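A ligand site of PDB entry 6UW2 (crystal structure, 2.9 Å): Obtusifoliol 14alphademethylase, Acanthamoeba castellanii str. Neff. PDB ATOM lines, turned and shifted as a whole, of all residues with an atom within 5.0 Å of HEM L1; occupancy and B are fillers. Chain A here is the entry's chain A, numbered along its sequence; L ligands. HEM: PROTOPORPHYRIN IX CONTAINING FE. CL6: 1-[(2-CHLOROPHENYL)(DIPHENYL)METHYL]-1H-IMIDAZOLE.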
ATOM      1  N   PHE A  68       8.603   0.518  25.770  1.00  0.00           N
ATOM      2  CA  PHE A  68       8.737  -0.841  25.199  1.00  0.00           C
ATOM      3  C   PHE A  68       8.312  -1.971  26.137  1.00  0.00           C
ATOM      4  O   PHE A  68       7.520  -2.835  25.741  1.00  0.00           O
ATOM      5  CB  PHE A  68      10.192  -1.075  24.763  1.00  0.00           C
ATOM      6  CG  PHE A  68      10.372  -2.269  23.883  1.00  0.00           C
ATOM      7  CD1 PHE A  68      10.110  -2.195  22.529  1.00  0.00           C
ATOM      8  CD2 PHE A  68      10.797  -3.473  24.406  1.00  0.00           C
ATOM      9  CE1 PHE A  68      10.264  -3.299  21.706  1.00  0.00           C
ATOM     10  CE2 PHE A  68      10.948  -4.590  23.587  1.00  0.00           C
ATOM     11  CZ  PHE A  68      10.680  -4.493  22.233  1.00  0.00           C
ATOM     12  N   GLN A  78       3.678  -8.286  18.799  1.00  0.00           N
ATOM     13  CA  GLN A  78       4.824  -9.139  18.484  1.00  0.00           C
ATOM     14  C   GLN A  78       4.770  -9.851  17.107  1.00  0.00           C
ATOM     15  O   GLN A  78       5.778 -10.424  16.686  1.00  0.00           O
ATOM     16  CB  GLN A  78       4.932 -10.226  19.546  1.00  0.00           C
ATOM     17  CG  GLN A  78       5.160  -9.734  20.951  1.00  0.00           C
ATOM     18  CD  GLN A  78       5.448 -10.902  21.864  1.00  0.00           C
ATOM     19  OE1 GLN A  78       4.577 -11.759  22.086  1.00  0.00           O
ATOM     20  NE2 GLN A  78       6.674 -10.975  22.373  1.00  0.00           N
ATOM     21  N   TYR A  82       8.134 -10.811  14.354  1.00  0.00           N
ATOM     22  CA  TYR A  82       8.516 -12.197  14.657  1.00  0.00           C
ATOM     23  C   TYR A  82       7.813 -13.200  13.733  1.00  0.00           C
ATOM     24  O   TYR A  82       7.608 -14.371  14.099  1.00  0.00           O
ATOM     25  CB  TYR A  82       8.229 -12.543  16.131  1.00  0.00           C
ATOM     26  CG  TYR A  82       9.030 -11.788  17.190  1.00  0.00           C
ATOM     27  CD1 TYR A  82      10.232 -11.095  16.888  1.00  0.00           C
ATOM     28  CD2 TYR A  82       8.617 -11.818  18.515  1.00  0.00           C
ATOM     29  CE1 TYR A  82      10.949 -10.434  17.859  1.00  0.00           C
ATOM     30  CE2 TYR A  82       9.332 -11.158  19.508  1.00  0.00           C
ATOM     31  CZ  TYR A  82      10.489 -10.455  19.185  1.00  0.00           C
ATOM     32  OH  TYR A  82      11.182  -9.800  20.195  1.00  0.00           O
ATOM     33  N   TYR A  95       3.929 -17.182  17.870  1.00  0.00           N
ATOM     34  CA  TYR A  95       3.684 -15.916  17.199  1.00  0.00           C
ATOM     35  C   TYR A  95       2.789 -16.090  15.968  1.00  0.00           C
ATOM     36  O   TYR A  95       2.287 -15.108  15.433  1.00  0.00           O
ATOM     37  CB  TYR A  95       5.007 -15.183  16.906  1.00  0.00           C
ATOM     38  CG  TYR A  95       5.830 -14.922  18.155  1.00  0.00           C
ATOM     39  CD1 TYR A  95       5.249 -14.373  19.302  1.00  0.00           C
ATOM     40  CD2 TYR A  95       7.178 -15.229  18.209  1.00  0.00           C
ATOM     41  CE1 TYR A  95       5.986 -14.140  20.459  1.00  0.00           C
ATOM     42  CE2 TYR A  95       7.923 -15.006  19.363  1.00  0.00           C
ATOM     43  CZ  TYR A  95       7.314 -14.452  20.485  1.00  0.00           C
ATOM     44  OH  TYR A  95       8.029 -14.207  21.641  1.00  0.00           O
ATOM     45  N   LEU A 106       1.860 -19.726  26.077  1.00  0.00           N
ATOM     46  CA  LEU A 106       2.868 -19.046  26.904  1.00  0.00           C
ATOM     47  C   LEU A 106       2.731 -19.374  28.407  1.00  0.00           C
ATOM     48  O   LEU A 106       3.743 -19.500  29.092  1.00  0.00           O
ATOM     49  CB  LEU A 106       2.823 -17.529  26.693  1.00  0.00           C
ATOM     50  CG  LEU A 106       3.385 -17.013  25.374  1.00  0.00           C
ATOM     51  CD1 LEU A 106       3.054 -15.531  25.237  1.00  0.00           C
ATOM     52  CD2 LEU A 106       4.887 -17.256  25.269  1.00  0.00           C
ATOM     53  N   ILE A 109       4.082 -23.024  28.568  1.00  0.00           N
ATOM     54  CA  ILE A 109       5.556 -22.936  28.540  1.00  0.00           C
ATOM     55  C   ILE A 109       6.128 -22.567  29.911  1.00  0.00           C
ATOM     56  O   ILE A 109       7.172 -23.092  30.332  1.00  0.00           O
ATOM     57  CB  ILE A 109       6.052 -21.916  27.490  1.00  0.00           C
ATOM     58  CG1 ILE A 109       5.832 -22.465  26.075  1.00  0.00           C
ATOM     59  CG2 ILE A 109       7.538 -21.591  27.648  1.00  0.00           C
ATOM     60  CD1 ILE A 109       6.097 -21.471  24.968  1.00  0.00           C
ATOM     61  N   LEU A 113       8.758 -24.630  32.572  1.00  0.00           N
ATOM     62  CA  LEU A 113      10.067 -24.075  32.971  1.00  0.00           C
ATOM     63  C   LEU A 113      10.015 -23.340  34.309  1.00  0.00           C
ATOM     64  O   LEU A 113      10.850 -22.470  34.582  1.00  0.00           O
ATOM     65  CB  LEU A 113      10.606 -23.149  31.860  1.00  0.00           C
ATOM     66  CG  LEU A 113      10.805 -23.841  30.506  1.00  0.00           C
ATOM     67  CD1 LEU A 113      10.927 -22.813  29.397  1.00  0.00           C
ATOM     68  CD2 LEU A 113      12.022 -24.765  30.509  1.00  0.00           C
ATOM     69  N   LEU A 160      13.234 -31.257  27.441  1.00  0.00           N
ATOM     70  CA  LEU A 160      12.118 -30.796  26.629  1.00  0.00           C
ATOM     71  C   LEU A 160      11.335 -31.993  26.092  1.00  0.00           C
ATOM     72  O   LEU A 160      10.123 -32.070  26.287  1.00  0.00           O
ATOM     73  CB  LEU A 160      12.610 -29.904  25.479  1.00  0.00           C
ATOM     74  CG  LEU A 160      13.613 -28.784  25.789  1.00  0.00           C
ATOM     75  CD1 LEU A 160      14.057 -28.121  24.481  1.00  0.00           C
ATOM     76  CD2 LEU A 160      13.032 -27.752  26.746  1.00  0.00           C
ATOM     77  N   LEU A 259      11.364 -24.095  21.863  1.00  0.00           N
ATOM     78  CA  LEU A 259      12.256 -24.184  23.025  1.00  0.00           C
ATOM     79  C   LEU A 259      13.590 -24.819  22.676  1.00  0.00           C
ATOM     80  O   LEU A 259      14.636 -24.449  23.238  1.00  0.00           O
ATOM     81  CB  LEU A 259      11.593 -24.986  24.141  1.00  0.00           C
ATOM     82  CG  LEU A 259      10.287 -24.404  24.671  1.00  0.00           C
ATOM     83  CD1 LEU A 259       9.559 -25.420  25.525  1.00  0.00           C
ATOM     84  CD2 LEU A 259      10.510 -23.144  25.477  1.00  0.00           C
ATOM     85  N   ALA A 262      15.633 -22.092  21.302  1.00  0.00           N
ATOM     86  CA  ALA A 262      16.044 -21.152  22.330  1.00  0.00           C
ATOM     87  C   ALA A 262      17.368 -21.594  22.919  1.00  0.00           C
ATOM     88  O   ALA A 262      18.330 -20.825  22.927  1.00  0.00           O
ATOM     89  CB  ALA A 262      14.984 -21.074  23.416  1.00  0.00           C
ATOM     90  N   GLY A 263      17.408 -22.857  23.383  1.00  0.00           N
ATOM     91  CA  GLY A 263      18.609 -23.467  23.966  1.00  0.00           C
ATOM     92  C   GLY A 263      19.827 -23.172  23.105  1.00  0.00           C
ATOM     93  O   GLY A 263      20.837 -22.621  23.595  1.00  0.00           O
ATOM     94  N   THR A 266      20.901 -19.238  22.057  1.00  0.00           N
ATOM     95  CA  THR A 266      21.258 -18.353  23.189  1.00  0.00           C
ATOM     96  C   THR A 266      22.063 -18.991  24.371  1.00  0.00           C
ATOM     97  O   THR A 266      23.186 -18.515  24.671  1.00  0.00           O
ATOM     98  CB  THR A 266      19.966 -17.742  23.747  1.00  0.00           C
ATOM     99  OG1 THR A 266      19.012 -18.785  23.975  1.00  0.00           O
ATOM    100  CG2 THR A 266      19.370 -16.777  22.770  1.00  0.00           C
ATOM    101  N   SER A 267      21.513 -20.034  25.032  1.00  0.00           N
ATOM    102  CA  SER A 267      22.201 -20.713  26.161  1.00  0.00           C
ATOM    103  C   SER A 267      23.581 -21.156  25.709  1.00  0.00           C
ATOM    104  O   SER A 267      24.596 -20.935  26.398  1.00  0.00           O
ATOM    105  CB  SER A 267      21.450 -21.953  26.648  1.00  0.00           C
ATOM    106  OG  SER A 267      20.202 -21.656  27.220  1.00  0.00           O
ATOM    107  N   THR A 270      26.118 -17.872  25.272  1.00  0.00           N
ATOM    108  CA  THR A 270      26.534 -17.199  26.509  1.00  0.00           C
ATOM    109  C   THR A 270      27.246 -18.202  27.386  1.00  0.00           C
ATOM    110  O   THR A 270      28.244 -17.877  28.038  1.00  0.00           O
ATOM    111  CB  THR A 270      25.362 -16.584  27.295  1.00  0.00           C
ATOM    112  OG1 THR A 270      24.152 -16.750  26.566  1.00  0.00           O
ATOM    113  CG2 THR A 270      25.640 -15.113  27.538  1.00  0.00           C
ATOM    114  N   LEU A 325      26.633 -12.243  29.560  1.00  0.00           N
ATOM    115  CA  LEU A 325      25.390 -11.851  28.954  1.00  0.00           C
ATOM    116  C   LEU A 325      25.334 -10.341  28.788  1.00  0.00           C
ATOM    117  O   LEU A 325      24.825  -9.850  27.791  1.00  0.00           O
ATOM    118  CB  LEU A 325      24.211 -12.381  29.762  1.00  0.00           C
ATOM    119  CG  LEU A 325      22.781 -12.181  29.226  1.00  0.00           C
ATOM    120  CD1 LEU A 325      22.601 -12.387  27.727  1.00  0.00           C
ATOM    121  CD2 LEU A 325      21.861 -13.125  29.978  1.00  0.00           C
ATOM    122  N   PRO A 330      23.267 -12.793  23.221  1.00  0.00           N
ATOM    123  CA  PRO A 330      23.058 -13.565  21.989  1.00  0.00           C
ATOM    124  C   PRO A 330      22.045 -12.991  21.002  1.00  0.00           C
ATOM    125  O   PRO A 330      22.226 -13.180  19.798  1.00  0.00           O
ATOM    126  CB  PRO A 330      22.567 -14.923  22.499  1.00  0.00           C
ATOM    127  CG  PRO A 330      22.037 -14.667  23.848  1.00  0.00           C
ATOM    128  CD  PRO A 330      22.894 -13.565  24.416  1.00  0.00           C
ATOM    129  N   LEU A 331      20.978 -12.365  21.482  1.00  0.00           N
ATOM    130  CA  LEU A 331      20.021 -11.695  20.594  1.00  0.00           C
ATOM    131  C   LEU A 331      20.321 -10.229  20.596  1.00  0.00           C
ATOM    132  O   LEU A 331      20.437  -9.630  21.676  1.00  0.00           O
ATOM    133  CB  LEU A 331      18.593 -11.927  21.027  1.00  0.00           C
ATOM    134  CG  LEU A 331      18.291 -13.412  21.249  1.00  0.00           C
ATOM    135  CD1 LEU A 331      16.795 -13.606  21.333  1.00  0.00           C
ATOM    136  CD2 LEU A 331      18.838 -14.323  20.151  1.00  0.00           C
ATOM    137  N   VAL A 334      15.276  -6.872  20.095  1.00  0.00           N
ATOM    138  CA  VAL A 334      13.909  -7.275  20.357  1.00  0.00           C
ATOM    139  C   VAL A 334      13.012  -6.182  19.772  1.00  0.00           C
ATOM    140  O   VAL A 334      13.444  -5.012  19.656  1.00  0.00           O
ATOM    141  CB  VAL A 334      13.643  -7.506  21.851  1.00  0.00           C
ATOM    142  CG1 VAL A 334      14.004  -8.935  22.220  1.00  0.00           C
ATOM    143  CG2 VAL A 334      14.410  -6.513  22.713  1.00  0.00           C
ATOM    144  N   ARG A 336       8.868  -4.730  18.438  1.00  0.00           N
ATOM    145  CA  ARG A 336       7.394  -4.666  18.395  1.00  0.00           C
ATOM    146  C   ARG A 336       6.930  -3.651  17.348  1.00  0.00           C
ATOM    147  O   ARG A 336       7.524  -2.586  17.233  1.00  0.00           O
ATOM    148  CB  ARG A 336       6.810  -4.214  19.738  1.00  0.00           C
ATOM    149  CG  ARG A 336       7.257  -4.987  20.970  1.00  0.00           C
ATOM    150  CD  ARG A 336       6.592  -6.348  21.104  1.00  0.00           C
ATOM    151  NE  ARG A 336       6.910  -6.982  22.391  1.00  0.00           N
ATOM    152  CZ  ARG A 336       8.031  -7.640  22.699  1.00  0.00           C
ATOM    153  NH1 ARG A 336       9.018  -7.777  21.836  1.00  0.00           N
ATOM    154  NH2 ARG A 336       8.161  -8.159  23.901  1.00  0.00           N
ATOM    155  N   VAL A 393      19.074  -5.751  30.335  1.00  0.00           N
ATOM    156  CA  VAL A 393      17.943  -6.248  29.515  1.00  0.00           C
ATOM    157  C   VAL A 393      18.210  -7.565  28.797  1.00  0.00           C
ATOM    158  O   VAL A 393      17.382  -7.975  27.981  1.00  0.00           O
ATOM    159  CB  VAL A 393      17.468  -5.201  28.462  1.00  0.00           C
ATOM    160  CG1 VAL A 393      16.377  -4.314  29.037  1.00  0.00           C
ATOM    161  CG2 VAL A 393      18.629  -4.356  27.947  1.00  0.00           C
ATOM    162  N   GLY A 394      19.311  -8.246  29.094  1.00  0.00           N
ATOM    163  CA  GLY A 394      19.661  -9.495  28.405  1.00  0.00           C
ATOM    164  C   GLY A 394      18.526 -10.510  28.208  1.00  0.00           C
ATOM    165  O   GLY A 394      18.456 -11.155  27.176  1.00  0.00           O
ATOM    166  N   PHE A 395      17.637 -10.621  29.206  1.00  0.00           N
ATOM    167  CA  PHE A 395      16.482 -11.512  29.147  1.00  0.00           C
ATOM    168  C   PHE A 395      15.168 -10.751  28.929  1.00  0.00           C
ATOM    169  O   PHE A 395      14.074 -11.299  29.160  1.00  0.00           O
ATOM    170  CB  PHE A 395      16.361 -12.289  30.455  1.00  0.00           C
ATOM    171  CG  PHE A 395      17.460 -13.266  30.696  1.00  0.00           C
ATOM    172  CD1 PHE A 395      17.489 -14.485  30.030  1.00  0.00           C
ATOM    173  CD2 PHE A 395      18.453 -12.994  31.631  1.00  0.00           C
ATOM    174  CE1 PHE A 395      18.482 -15.393  30.259  1.00  0.00           C
ATOM    175  CE2 PHE A 395      19.460 -13.903  31.866  1.00  0.00           C
ATOM    176  CZ  PHE A 395      19.484 -15.097  31.177  1.00  0.00           C
ATOM    177  N   GLY A 396      15.273  -9.496  28.503  1.00  0.00           N
ATOM    178  CA  GLY A 396      14.109  -8.672  28.193  1.00  0.00           C
ATOM    179  C   GLY A 396      13.433  -8.210  29.462  1.00  0.00           C
ATOM    180  O   GLY A 396      14.080  -8.077  30.509  1.00  0.00           O
ATOM    181  N   ARG A 399       5.629  -8.092  30.289  1.00  0.00           N
ATOM    182  CA  ARG A 399       4.672  -9.138  29.934  1.00  0.00           C
ATOM    183  C   ARG A 399       5.398 -10.277  29.223  1.00  0.00           C
ATOM    184  O   ARG A 399       5.056 -11.426  29.458  1.00  0.00           O
ATOM    185  CB  ARG A 399       3.503  -8.560  29.101  1.00  0.00           C
ATOM    186  CG  ARG A 399       2.486  -9.553  28.473  1.00  0.00           C
ATOM    187  CD  ARG A 399       1.596 -10.242  29.502  1.00  0.00           C
ATOM    188  NE  ARG A 399       0.871 -11.435  29.010  1.00  0.00           N
ATOM    189  CZ  ARG A 399       1.370 -12.686  28.906  1.00  0.00           C
ATOM    190  NH1 ARG A 399       2.635 -12.978  29.196  1.00  0.00           N
ATOM    191  NH2 ARG A 399       0.574 -13.670  28.486  1.00  0.00           N
ATOM    192  N   HIS A 400       6.422  -9.968  28.407  1.00  0.00           N
ATOM    193  CA  HIS A 400       7.152 -10.977  27.613  1.00  0.00           C
ATOM    194  C   HIS A 400       8.659 -10.987  27.842  1.00  0.00           C
ATOM    195  O   HIS A 400       9.424 -11.047  26.896  1.00  0.00           O
ATOM    196  CB  HIS A 400       6.903 -10.745  26.121  1.00  0.00           C
ATOM    197  CG  HIS A 400       5.472 -10.813  25.736  1.00  0.00           C
ATOM    198  ND1 HIS A 400       4.783  -9.719  25.278  1.00  0.00           N
ATOM    199  CD2 HIS A 400       4.585 -11.837  25.731  1.00  0.00           C
ATOM    200  CE1 HIS A 400       3.536 -10.059  25.002  1.00  0.00           C
ATOM    201  NE2 HIS A 400       3.392 -11.346  25.277  1.00  0.00           N
ATOM    202  N   GLY A 401       9.076 -10.941  29.096  1.00  0.00           N
ATOM    203  CA  GLY A 401      10.479 -11.218  29.446  1.00  0.00           C
ATOM    204  C   GLY A 401      10.738 -12.717  29.367  1.00  0.00           C
ATOM    205  O   GLY A 401       9.798 -13.510  29.320  1.00  0.00           O
ATOM    206  N   CYS A 402      11.998 -13.119  29.378  1.00  0.00           N
ATOM    207  CA  CYS A 402      12.324 -14.526  29.130  1.00  0.00           C
ATOM    208  C   CYS A 402      11.718 -15.487  30.159  1.00  0.00           C
ATOM    209  O   CYS A 402      11.637 -15.133  31.326  1.00  0.00           O
ATOM    210  CB  CYS A 402      13.842 -14.718  29.102  1.00  0.00           C
ATOM    211  SG  CYS A 402      14.341 -16.337  28.502  1.00  0.00           S
ATOM    212  N   MET A 403      11.278 -16.656  29.723  1.00  0.00           N
ATOM    213  CA  MET A 403      10.748 -17.683  30.614  1.00  0.00           C
ATOM    214  C   MET A 403      11.758 -18.776  30.888  1.00  0.00           C
ATOM    215  O   MET A 403      11.495 -19.680  31.687  1.00  0.00           O
ATOM    216  CB  MET A 403       9.495 -18.323  30.030  1.00  0.00           C
ATOM    217  CG  MET A 403       8.267 -17.477  30.155  1.00  0.00           C
ATOM    218  SD  MET A 403       6.830 -18.438  29.636  1.00  0.00           S
ATOM    219  CE  MET A 403       5.764 -17.183  28.911  1.00  0.00           C
ATOM    220  N   GLY A 404      12.909 -18.737  30.227  1.00  0.00           N
ATOM    221  CA  GLY A 404      13.940 -19.753  30.423  1.00  0.00           C
ATOM    222  C   GLY A 404      15.132 -19.283  31.221  1.00  0.00           C
ATOM    223  O   GLY A 404      16.093 -20.031  31.386  1.00  0.00           O
ATOM    224  N   PHE A 407      16.234 -21.707  33.800  1.00  0.00           N
ATOM    225  CA  PHE A 407      16.750 -22.871  33.074  1.00  0.00           C
ATOM    226  C   PHE A 407      18.156 -22.617  32.531  1.00  0.00           C
ATOM    227  O   PHE A 407      19.025 -23.470  32.645  1.00  0.00           O
ATOM    228  CB  PHE A 407      15.806 -23.264  31.932  1.00  0.00           C
ATOM    229  CG  PHE A 407      16.285 -24.439  31.127  1.00  0.00           C
ATOM    230  CD1 PHE A 407      17.219 -24.270  30.101  1.00  0.00           C
ATOM    231  CD2 PHE A 407      15.830 -25.706  31.398  1.00  0.00           C
ATOM    232  CE1 PHE A 407      17.682 -25.351  29.368  1.00  0.00           C
ATOM    233  CE2 PHE A 407      16.268 -26.789  30.667  1.00  0.00           C
ATOM    234  CZ  PHE A 407      17.207 -26.611  29.651  1.00  0.00           C
ATOM    235  N   ALA A 408      18.359 -21.436  31.932  1.00  0.00           N
ATOM    236  CA  ALA A 408      19.643 -21.053  31.315  1.00  0.00           C
ATOM    237  C   ALA A 408      20.762 -20.866  32.320  1.00  0.00           C
ATOM    238  O   ALA A 408      21.838 -21.439  32.177  1.00  0.00           O
ATOM    239  CB  ALA A 408      19.485 -19.770  30.511  1.00  0.00           C
ATOM    240  N   ILE A 412      23.911 -23.307  32.405  1.00  0.00           N
ATOM    241  CA  ILE A 412      25.242 -22.752  32.196  1.00  0.00           C
ATOM    242  C   ILE A 412      26.057 -22.948  33.472  1.00  0.00           C
ATOM    243  O   ILE A 412      27.230 -23.264  33.392  1.00  0.00           O
ATOM    244  CB  ILE A 412      25.194 -21.259  31.765  1.00  0.00           C
ATOM    245  CG1 ILE A 412      24.450 -21.099  30.439  1.00  0.00           C
ATOM    246  CG2 ILE A 412      26.608 -20.699  31.597  1.00  0.00           C
ATOM    247  CD1 ILE A 412      23.917 -19.696  30.242  1.00  0.00           C
HETATM  248  CHA HEM L   1      11.882 -14.502  25.507  1.00  0.00           C
HETATM  249  CHB HEM L   1      16.608 -13.862  26.035  1.00  0.00           C
HETATM  250  CHC HEM L   1      17.179 -18.594  26.885  1.00  0.00           C
HETATM  251  CHD HEM L   1      12.362 -19.193  26.454  1.00  0.00           C
HETATM  252  C1A HEM L   1      13.115 -13.932  25.573  1.00  0.00           C
HETATM  253  C2A HEM L   1      13.364 -12.570  25.333  1.00  0.00           C
HETATM  254  C3A HEM L   1      14.699 -12.360  25.488  1.00  0.00           C
HETATM  255  C4A HEM L   1      15.264 -13.623  25.815  1.00  0.00           C
HETATM  256  CMA HEM L   1      15.418 -11.032  25.331  1.00  0.00           C
HETATM  257  CAA HEM L   1      12.336 -11.516  25.021  1.00  0.00           C
HETATM  258  CBA HEM L   1      11.849 -11.569  23.582  1.00  0.00           C
HETATM  259  CGA HEM L   1      10.845 -10.458  23.371  1.00  0.00           C
HETATM  260  O1A HEM L   1       9.741 -10.695  22.837  1.00  0.00           O
HETATM  261  O2A HEM L   1      11.119  -9.282  23.728  1.00  0.00           O
HETATM  262  C1B HEM L   1      17.179 -15.098  26.330  1.00  0.00           C
HETATM  263  C2B HEM L   1      18.584 -15.271  26.560  1.00  0.00           C
HETATM  264  C3B HEM L   1      18.772 -16.599  26.786  1.00  0.00           C
HETATM  265  C4B HEM L   1      17.422 -17.229  26.698  1.00  0.00           C
HETATM  266  CMB HEM L   1      19.653 -14.200  26.537  1.00  0.00           C
HETATM  267  CAB HEM L   1      20.022 -17.295  27.148  1.00  0.00           C
HETATM  268  CBB HEM L   1      21.148 -16.723  27.584  1.00  0.00           C
HETATM  269  C1C HEM L   1      15.915 -19.206  26.834  1.00  0.00           C
HETATM  270  C2C HEM L   1      15.657 -20.596  26.979  1.00  0.00           C
HETATM  271  C3C HEM L   1      14.269 -20.760  26.865  1.00  0.00           C
HETATM  272  C4C HEM L   1      13.706 -19.462  26.651  1.00  0.00           C
HETATM  273  CMC HEM L   1      16.694 -21.673  27.246  1.00  0.00           C
HETATM  274  CAC HEM L   1      13.434 -21.981  26.911  1.00  0.00           C
HETATM  275  CBC HEM L   1      13.867 -23.230  26.964  1.00  0.00           C
HETATM  276  C1D HEM L   1      11.895 -17.926  26.152  1.00  0.00           C
HETATM  277  C2D HEM L   1      10.447 -17.684  25.925  1.00  0.00           C
HETATM  278  C3D HEM L   1      10.309 -16.369  25.688  1.00  0.00           C
HETATM  279  C4D HEM L   1      11.684 -15.846  25.737  1.00  0.00           C
HETATM  280  CMD HEM L   1       9.282 -18.670  25.968  1.00  0.00           C
HETATM  281  CAD HEM L   1       8.999 -15.680  25.340  1.00  0.00           C
HETATM  282  CBD HEM L   1       8.462 -14.515  26.171  1.00  0.00           C
HETATM  283  CGD HEM L   1       7.027 -14.315  25.702  1.00  0.00           C
HETATM  284  O1D HEM L   1       6.771 -13.914  24.530  1.00  0.00           O
HETATM  285  O2D HEM L   1       6.089 -14.585  26.503  1.00  0.00           O
HETATM  286  NA  HEM L   1      14.282 -14.592  25.808  1.00  0.00           N
HETATM  287  NB  HEM L   1      16.554 -16.281  26.410  1.00  0.00           N
HETATM  288  NC  HEM L   1      14.729 -18.568  26.566  1.00  0.00           N
HETATM  289  ND  HEM L   1      12.600 -16.790  26.019  1.00  0.00           N
HETATM  290 FE   HEM L   1      14.484 -16.547  26.206  1.00  0.00          FE
HETATM  291 CLAY CL6 L   2      11.376 -15.989  18.163  1.00  0.00          CL
HETATM  292  CAX CL6 L   2      12.287 -14.893  19.246  1.00  0.00           C
HETATM  293  CAV CL6 L   2      12.237 -13.521  18.953  1.00  0.00           C
HETATM  294  CAT CL6 L   2      12.926 -12.600  19.732  1.00  0.00           C
HETATM  295  CAS CL6 L   2      13.643 -13.039  20.825  1.00  0.00           C
HETATM  296  CAU CL6 L   2      13.714 -14.392  21.164  1.00  0.00           C
HETATM  297  CAW CL6 L   2      13.053 -15.403  20.431  1.00  0.00           C
HETATM  298  CAR CL6 L   2      13.179 -16.889  20.787  1.00  0.00           C
HETATM  299  CAC CL6 L   2      11.905 -17.630  21.183  1.00  0.00           C
HETATM  300  CAE CL6 L   2      12.005 -18.966  21.619  1.00  0.00           C
HETATM  301  CAF CL6 L   2      10.894 -19.731  22.008  1.00  0.00           C
HETATM  302  CAD CL6 L   2       9.633 -19.169  22.003  1.00  0.00           C
HETATM  303  CAB CL6 L   2       9.510 -17.839  21.583  1.00  0.00           C
HETATM  304  CAA CL6 L   2      10.622 -17.073  21.194  1.00  0.00           C
HETATM  305  NAO CL6 L   2      14.130 -17.038  21.984  1.00  0.00           N
HETATM  306  CAM CL6 L   2      13.688 -16.883  23.236  1.00  0.00           C
HETATM  307  NAN CL6 L   2      14.738 -17.056  24.081  1.00  0.00           N
HETATM  308  CAQ CL6 L   2      15.831 -17.320  23.332  1.00  0.00           C
HETATM  309  CAP CL6 L   2      15.465 -17.311  21.997  1.00  0.00           C
HETATM  310  CAL CL6 L   2      13.788 -17.558  19.539  1.00  0.00           C
HETATM  311  CAK CL6 L   2      13.223 -18.678  18.875  1.00  0.00           C
HETATM  312  CAI CL6 L   2      13.809 -19.250  17.751  1.00  0.00           C
HETATM  313  CAG CL6 L   2      14.988 -18.717  17.239  1.00  0.00           C
HETATM  314  CAH CL6 L   2      15.565 -17.607  17.854  1.00  0.00           C
HETATM  315  CAJ CL6 L   2      14.966 -17.034  18.973  1.00  0.00           C
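Merely in contact with HEM L1: Leu 106, Ile 109, Leu 113, Leu 259, Ala 262, Thr 266, Ser 267, Thr 270, Leu 325, Pro 330, Val 334, Gly 394, Phe 395, Gly 396, His 400, Gly 401, Met 403, Gly 404 and Phe 407.
The nearest printed residue that does not touch HEM L1 is Gly 263 (4.1 Å).
A nitrogen (NAN) of CL6 L2 binds an iron atom (FE) of HEM L1 (2.2 Å).
The backbone NH (N) of Cys 402 lies within hydrogen-bond range of the backbone carbonyl oxygen (O) of Phe 395 (2.8 Å).
The side-chain sulfur of Cys 402 lies close to the backbone NH of Gly 404 (3.3 Å).
The side-chain amide oxygen of Gln 78 is in hydrogen-bond range of a ring nitrogen (NE2) of His 400.
The side-chain hydroxyl of Tyr 82 is in hydrogen-bond range of the guanidinium group of Arg 336, at 3.4 Å.
OG1 of Thr 270 sits at hydrogen-bond distance from O of Thr 266 (2.8 Å).
FE of HEM L1 is bound by SG of Cys 402, at 2.3 Å.
O1A of HEM L1 sits at hydrogen-bond distance from NE2 of Gln 78 (3.1 Å).
The side-chain hydroxyl of Tyr 82 sits at hydrogen-bond distance from an oxygen (O1A) of HEM L1 (3.1 Å).
OH of Tyr 95 sits at hydrogen-bond distance from O1D of HEM L1.
An oxygen (O2A) of HEM L1 is in salt-bridge range of the guanidinium group of Arg 336.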
